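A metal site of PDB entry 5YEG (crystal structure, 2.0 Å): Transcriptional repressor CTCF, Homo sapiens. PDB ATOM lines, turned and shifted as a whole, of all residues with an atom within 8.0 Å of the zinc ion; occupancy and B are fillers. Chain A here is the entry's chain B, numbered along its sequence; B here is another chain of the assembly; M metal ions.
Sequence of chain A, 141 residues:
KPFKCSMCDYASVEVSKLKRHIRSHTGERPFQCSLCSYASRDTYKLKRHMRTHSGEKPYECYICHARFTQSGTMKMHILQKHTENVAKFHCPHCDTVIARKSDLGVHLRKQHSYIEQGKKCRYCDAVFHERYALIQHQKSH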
ATOM      1  N   HIS A  90     -17.037 -26.281  31.405  1.00  0.00           N
ATOM      2  CA  HIS A  90     -17.379 -25.192  30.509  1.00  0.00           C
ATOM      3  C   HIS A  90     -16.457 -25.268  29.313  1.00  0.00           C
ATOM      4  O   HIS A  90     -15.234 -25.301  29.468  1.00  0.00           O
ATOM      5  CB  HIS A  90     -17.243 -23.825  31.176  1.00  0.00           C
ATOM      6  CG  HIS A  90     -18.210 -23.577  32.285  1.00  0.00           C
ATOM      7  ND1 HIS A  90     -18.131 -24.226  33.507  1.00  0.00           N
ATOM      8  CD2 HIS A  90     -19.272 -22.755  32.367  1.00  0.00           C
ATOM      9  CE1 HIS A  90     -19.123 -23.815  34.279  1.00  0.00           C
ATOM     10  NE2 HIS A  90     -19.827 -22.918  33.617  1.00  0.00           N
ATOM     11  N   CYS A  91     -17.038 -25.340  28.130  1.00  0.00           N
ATOM     12  CA  CYS A  91     -16.204 -25.321  26.949  1.00  0.00           C
ATOM     13  C   CYS A  91     -15.432 -24.001  26.872  1.00  0.00           C
ATOM     14  O   CYS A  91     -16.034 -22.935  27.071  1.00  0.00           O
ATOM     15  CB  CYS A  91     -17.057 -25.495  25.711  1.00  0.00           C
ATOM     16  SG  CYS A  91     -16.019 -25.356  24.311  1.00  0.00           S
ATOM     17  N   PRO A  92     -14.129 -24.024  26.583  1.00  0.00           N
ATOM     18  CA  PRO A  92     -13.350 -22.772  26.557  1.00  0.00           C
ATOM     19  C   PRO A  92     -13.669 -21.874  25.383  1.00  0.00           C
ATOM     20  O   PRO A  92     -13.412 -20.662  25.458  1.00  0.00           O
ATOM     21  CB  PRO A  92     -11.889 -23.250  26.490  1.00  0.00           C
ATOM     22  CG  PRO A  92     -11.940 -24.748  26.557  1.00  0.00           C
ATOM     23  CD  PRO A  92     -13.309 -25.190  26.231  1.00  0.00           C
ATOM     24  N   HIS A  93     -14.220 -22.428  24.309  1.00  0.00           N
ATOM     25  CA  HIS A  93     -14.404 -21.713  23.055  1.00  0.00           C
ATOM     26  C   HIS A  93     -15.835 -21.247  22.806  1.00  0.00           C
ATOM     27  O   HIS A  93     -16.064 -20.558  21.816  1.00  0.00           O
ATOM     28  CB  HIS A  93     -13.934 -22.577  21.874  1.00  0.00           C
ATOM     29  CG  HIS A  93     -12.551 -23.117  22.032  1.00  0.00           C
ATOM     30  ND1 HIS A  93     -12.241 -24.447  21.866  1.00  0.00           N
ATOM     31  CD2 HIS A  93     -11.375 -22.507  22.347  1.00  0.00           C
ATOM     32  CE1 HIS A  93     -10.961 -24.643  22.075  1.00  0.00           C
ATOM     33  NE2 HIS A  93     -10.406 -23.476  22.364  1.00  0.00           N
ATOM     34  N   CYS A  94     -16.805 -21.635  23.629  1.00  0.00           N
ATOM     35  CA  CYS A  94     -18.200 -21.207  23.441  1.00  0.00           C
ATOM     36  C   CYS A  94     -18.922 -21.327  24.768  1.00  0.00           C
ATOM     37  O   CYS A  94     -18.312 -21.654  25.797  1.00  0.00           O
ATOM     38  CB  CYS A  94     -18.925 -22.001  22.347  1.00  0.00           C
ATOM     39  SG  CYS A  94     -19.395 -23.728  22.801  1.00  0.00           S
ATOM     40  N   ASP A  95     -20.245 -21.136  24.734  1.00  0.00           N
ATOM     41  CA  ASP A  95     -21.022 -21.026  25.974  1.00  0.00           C
ATOM     42  C   ASP A  95     -21.432 -22.363  26.561  1.00  0.00           C
ATOM     43  O   ASP A  95     -21.947 -22.383  27.681  1.00  0.00           O
ATOM     44  CB  ASP A  95     -22.280 -20.181  25.731  1.00  0.00           C
ATOM     45  N   THR A  96     -21.198 -23.477  25.861  1.00  0.00           N
ATOM     46  CA  THR A  96     -21.741 -24.756  26.277  1.00  0.00           C
ATOM     47  C   THR A  96     -21.063 -25.288  27.540  1.00  0.00           C
ATOM     48  O   THR A  96     -19.839 -25.244  27.685  1.00  0.00           O
ATOM     49  CB  THR A  96     -21.581 -25.772  25.155  1.00  0.00           C
ATOM     50  OG1 THR A  96     -22.178 -25.240  23.969  1.00  0.00           O
ATOM     51  CG2 THR A  96     -22.267 -27.096  25.504  1.00  0.00           C
ATOM     52  N   VAL A  97     -21.878 -25.829  28.443  1.00  0.00           N
ATOM     53  CA  VAL A  97     -21.394 -26.474  29.652  1.00  0.00           C
ATOM     54  C   VAL A  97     -21.741 -27.957  29.555  1.00  0.00           C
ATOM     55  O   VAL A  97     -22.881 -28.307  29.242  1.00  0.00           O
ATOM     56  CB  VAL A  97     -21.996 -25.840  30.913  1.00  0.00           C
ATOM     57  CG1 VAL A  97     -21.388 -26.444  32.175  1.00  0.00           C
ATOM     58  CG2 VAL A  97     -21.846 -24.326  30.861  1.00  0.00           C
ATOM     59  N   ILE A  98     -20.789 -28.818  29.868  1.00  0.00           N
ATOM     60  CA  ILE A  98     -20.918 -30.256  29.650  1.00  0.00           C
ATOM     61  C   ILE A  98     -20.539 -30.995  30.930  1.00  0.00           C
ATOM     62  O   ILE A  98     -19.555 -30.641  31.587  1.00  0.00           O
ATOM     63  CB  ILE A  98     -20.049 -30.716  28.462  1.00  0.00           C
ATOM     64  CG1 ILE A  98     -20.609 -30.135  27.162  1.00  0.00           C
ATOM     65  CG2 ILE A  98     -19.945 -32.221  28.414  1.00  0.00           C
ATOM     66  CD1 ILE A  98     -19.658 -30.224  26.007  1.00  0.00           C
ATOM     67  N   LEU A 104     -17.043 -33.395  26.935  1.00  0.00           N
ATOM     68  CA  LEU A 104     -16.430 -32.169  26.458  1.00  0.00           C
ATOM     69  C   LEU A 104     -15.409 -32.482  25.379  1.00  0.00           C
ATOM     70  O   LEU A 104     -15.284 -31.745  24.402  1.00  0.00           O
ATOM     71  CB  LEU A 104     -15.793 -31.386  27.603  1.00  0.00           C
ATOM     72  CG  LEU A 104     -14.926 -30.198  27.138  1.00  0.00           C
ATOM     73  CD1 LEU A 104     -15.770 -29.166  26.388  1.00  0.00           C
ATOM     74  CD2 LEU A 104     -14.186 -29.529  28.300  1.00  0.00           C
ATOM     75  N   HIS A 107     -17.283 -32.943  22.157  1.00  0.00           N
ATOM     76  CA  HIS A 107     -17.659 -31.605  21.727  1.00  0.00           C
ATOM     77  C   HIS A 107     -16.472 -30.878  21.106  1.00  0.00           C
ATOM     78  O   HIS A 107     -16.618 -30.201  20.083  1.00  0.00           O
ATOM     79  CB  HIS A 107     -18.206 -30.843  22.936  1.00  0.00           C
ATOM     80  CG  HIS A 107     -18.419 -29.379  22.706  1.00  0.00           C
ATOM     81  ND1 HIS A 107     -19.669 -28.833  22.487  1.00  0.00           N
ATOM     82  CD2 HIS A 107     -17.556 -28.339  22.683  1.00  0.00           C
ATOM     83  CE1 HIS A 107     -19.556 -27.529  22.335  1.00  0.00           C
ATOM     84  NE2 HIS A 107     -18.290 -27.203  22.447  1.00  0.00           N
ATOM     85  N   LEU A 108     -15.303 -31.001  21.720  1.00  0.00           N
ATOM     86  CA  LEU A 108     -14.084 -30.421  21.183  1.00  0.00           C
ATOM     87  C   LEU A 108     -13.820 -30.917  19.767  1.00  0.00           C
ATOM     88  O   LEU A 108     -13.572 -30.122  18.852  1.00  0.00           O
ATOM     89  CB  LEU A 108     -12.899 -30.784  22.066  1.00  0.00           C
ATOM     90  CG  LEU A 108     -12.276 -29.747  22.977  1.00  0.00           C
ATOM     91  CD1 LEU A 108     -13.327 -28.765  23.462  1.00  0.00           C
ATOM     92  CD2 LEU A 108     -11.612 -30.471  24.150  1.00  0.00           C
ATOM     93  N   GLN A 111     -16.959 -29.688  17.323  1.00  0.00           N
ATOM     94  CA  GLN A 111     -17.273 -28.269  17.161  1.00  0.00           C
ATOM     95  C   GLN A 111     -16.052 -27.382  16.981  1.00  0.00           C
ATOM     96  O   GLN A 111     -16.182 -26.284  16.416  1.00  0.00           O
ATOM     97  CB  GLN A 111     -18.074 -27.753  18.356  1.00  0.00           C
ATOM     98  CG  GLN A 111     -19.222 -28.643  18.788  1.00  0.00           C
ATOM     99  CD  GLN A 111     -20.270 -28.785  17.698  1.00  0.00           C
ATOM    100  OE1 GLN A 111     -20.414 -27.912  16.852  1.00  0.00           O
ATOM    101  NE2 GLN A 111     -21.031 -29.879  17.735  1.00  0.00           N
ATOM    102  N   HIS A 112     -14.881 -27.808  17.438  1.00  0.00           N
ATOM    103  CA  HIS A 112     -13.754 -26.894  17.493  1.00  0.00           C
ATOM    104  C   HIS A 112     -12.491 -27.447  16.842  1.00  0.00           C
ATOM    105  O   HIS A 112     -11.398 -26.969  17.158  1.00  0.00           O
ATOM    106  CB  HIS A 112     -13.441 -26.496  18.937  1.00  0.00           C
ATOM    107  CG  HIS A 112     -14.612 -25.943  19.685  1.00  0.00           C
ATOM    108  ND1 HIS A 112     -15.324 -24.838  19.255  1.00  0.00           N
ATOM    109  CD2 HIS A 112     -15.165 -26.301  20.871  1.00  0.00           C
ATOM    110  CE1 HIS A 112     -16.292 -24.576  20.117  1.00  0.00           C
ATOM    111  NE2 HIS A 112     -16.189 -25.429  21.138  1.00  0.00           N
ATOM    112  N   GLU A 130     -13.589 -24.026  11.110  1.00  0.00           N
ATOM    113  CA  GLU A 130     -14.109 -24.590  12.343  1.00  0.00           C
ATOM    114  C   GLU A 130     -15.628 -24.650  12.286  1.00  0.00           C
ATOM    115  O   GLU A 130     -16.278 -23.690  11.846  1.00  0.00           O
ATOM    116  CB  GLU A 130     -13.667 -23.762  13.559  1.00  0.00           C
ATOM    117  CG  GLU A 130     -14.378 -24.120  14.832  1.00  0.00           C
ATOM    118  CD  GLU A 130     -13.730 -23.547  16.067  1.00  0.00           C
ATOM    119  OE1 GLU A 130     -14.481 -23.190  17.010  1.00  0.00           O
ATOM    120  OE2 GLU A 130     -12.487 -23.415  16.092  1.00  0.00           O
ATOM    121  N   TYR A 132     -17.866 -24.637  14.770  1.00  0.00           N
ATOM    122  CA  TYR A 132     -18.528 -23.675  15.639  1.00  0.00           C
ATOM    123  C   TYR A 132     -18.599 -22.304  14.980  1.00  0.00           C
ATOM    124  O   TYR A 132     -19.673 -21.681  14.908  1.00  0.00           O
ATOM    125  CB  TYR A 132     -17.814 -23.574  16.988  1.00  0.00           C
ATOM    126  CG  TYR A 132     -18.385 -22.477  17.852  1.00  0.00           C
ATOM    127  CD1 TYR A 132     -19.639 -22.597  18.427  1.00  0.00           C
ATOM    128  CD2 TYR A 132     -17.672 -21.303  18.061  1.00  0.00           C
ATOM    129  CE1 TYR A 132     -20.162 -21.582  19.216  1.00  0.00           C
ATOM    130  CE2 TYR A 132     -18.179 -20.281  18.841  1.00  0.00           C
ATOM    131  CZ  TYR A 132     -19.426 -20.423  19.412  1.00  0.00           C
ATOM    132  OH  TYR A 132     -19.940 -19.412  20.190  1.00  0.00           O
ATOM    133  P    DA B   7     -22.572 -31.139  22.810  1.00  0.00           P
ATOM    134  OP1  DA B   7     -22.155 -29.722  22.753  1.00  0.00           O
ATOM    135  OP2  DA B   7     -21.618 -32.204  22.397  1.00  0.00           O
ATOM    136  O5'  DA B   7     -23.083 -31.439  24.298  1.00  0.00           O
ATOM    137  C5'  DA B   7     -24.139 -30.679  24.836  1.00  0.00           C
ATOM    138  C4'  DA B   7     -24.996 -31.528  25.756  1.00  0.00           C
ATOM    139  O4'  DA B   7     -25.652 -32.567  24.998  1.00  0.00           O
ATOM    140  C3'  DA B   7     -24.253 -32.235  26.887  1.00  0.00           C
ATOM    141  O3'  DA B   7     -25.101 -32.259  28.019  1.00  0.00           O
ATOM    142  C2'  DA B   7     -24.018 -33.639  26.310  1.00  0.00           C
ATOM    143  C1'  DA B   7     -25.288 -33.840  25.493  1.00  0.00           C
ATOM    144  N9   DA B   7     -25.136 -34.737  24.351  1.00  0.00           N
ATOM    145  C8   DA B   7     -24.192 -34.649  23.366  1.00  0.00           C
ATOM    146  N7   DA B   7     -24.319 -35.570  22.422  1.00  0.00           N
ATOM    147  C5   DA B   7     -25.435 -36.281  22.795  1.00  0.00           C
ATOM    148  C6   DA B   7     -26.103 -37.373  22.214  1.00  0.00           C
ATOM    149  N6   DA B   7     -25.710 -37.946  21.075  1.00  0.00           N
ATOM    150  N1   DA B   7     -27.201 -37.869  22.847  1.00  0.00           N
ATOM    151  C2   DA B   7     -27.600 -37.284  23.985  1.00  0.00           C
ATOM    152  N3   DA B   7     -27.047 -36.245  24.628  1.00  0.00           N
ATOM    153  C4   DA B   7     -25.970 -35.785  23.976  1.00  0.00           C
HETATM  154 ZN    ZN M   1     -17.711 -25.195  22.604  1.00  0.00          ZN
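The zinc ion is bound by NE2 of His 107 (2.1 Å), NE2 of His 112 (2.1 Å), SG of Cys 94 (2.2 Å) and SG of Cys 91 (2.4 Å).
The zinc ion has four donor atoms within binding distance.
A ring nitrogen (ND1) of His 112 is in hydrogen-bond range of the side-chain carboxylate (OE1) of Glu 130.
The backbone NH (N) of Cys 91 lies within hydrogen-bond range of the backbone carbonyl oxygen (O) of Thr 96, 2.8 Å away.
The side-chain hydroxyl (OG1) of Thr 96 lies close to the side-chain sulfur (SG) of Cys 94, 3.4 Å away.
OP1 of DA 7 of chain B is in hydrogen-bond range of a ring nitrogen (ND1) of His 107, at 2.7 Å.
SG of Cys 91 sits close to N of His 93.
Along chain A the residues within 4 Å of the zinc ion span positions 91 to 112.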
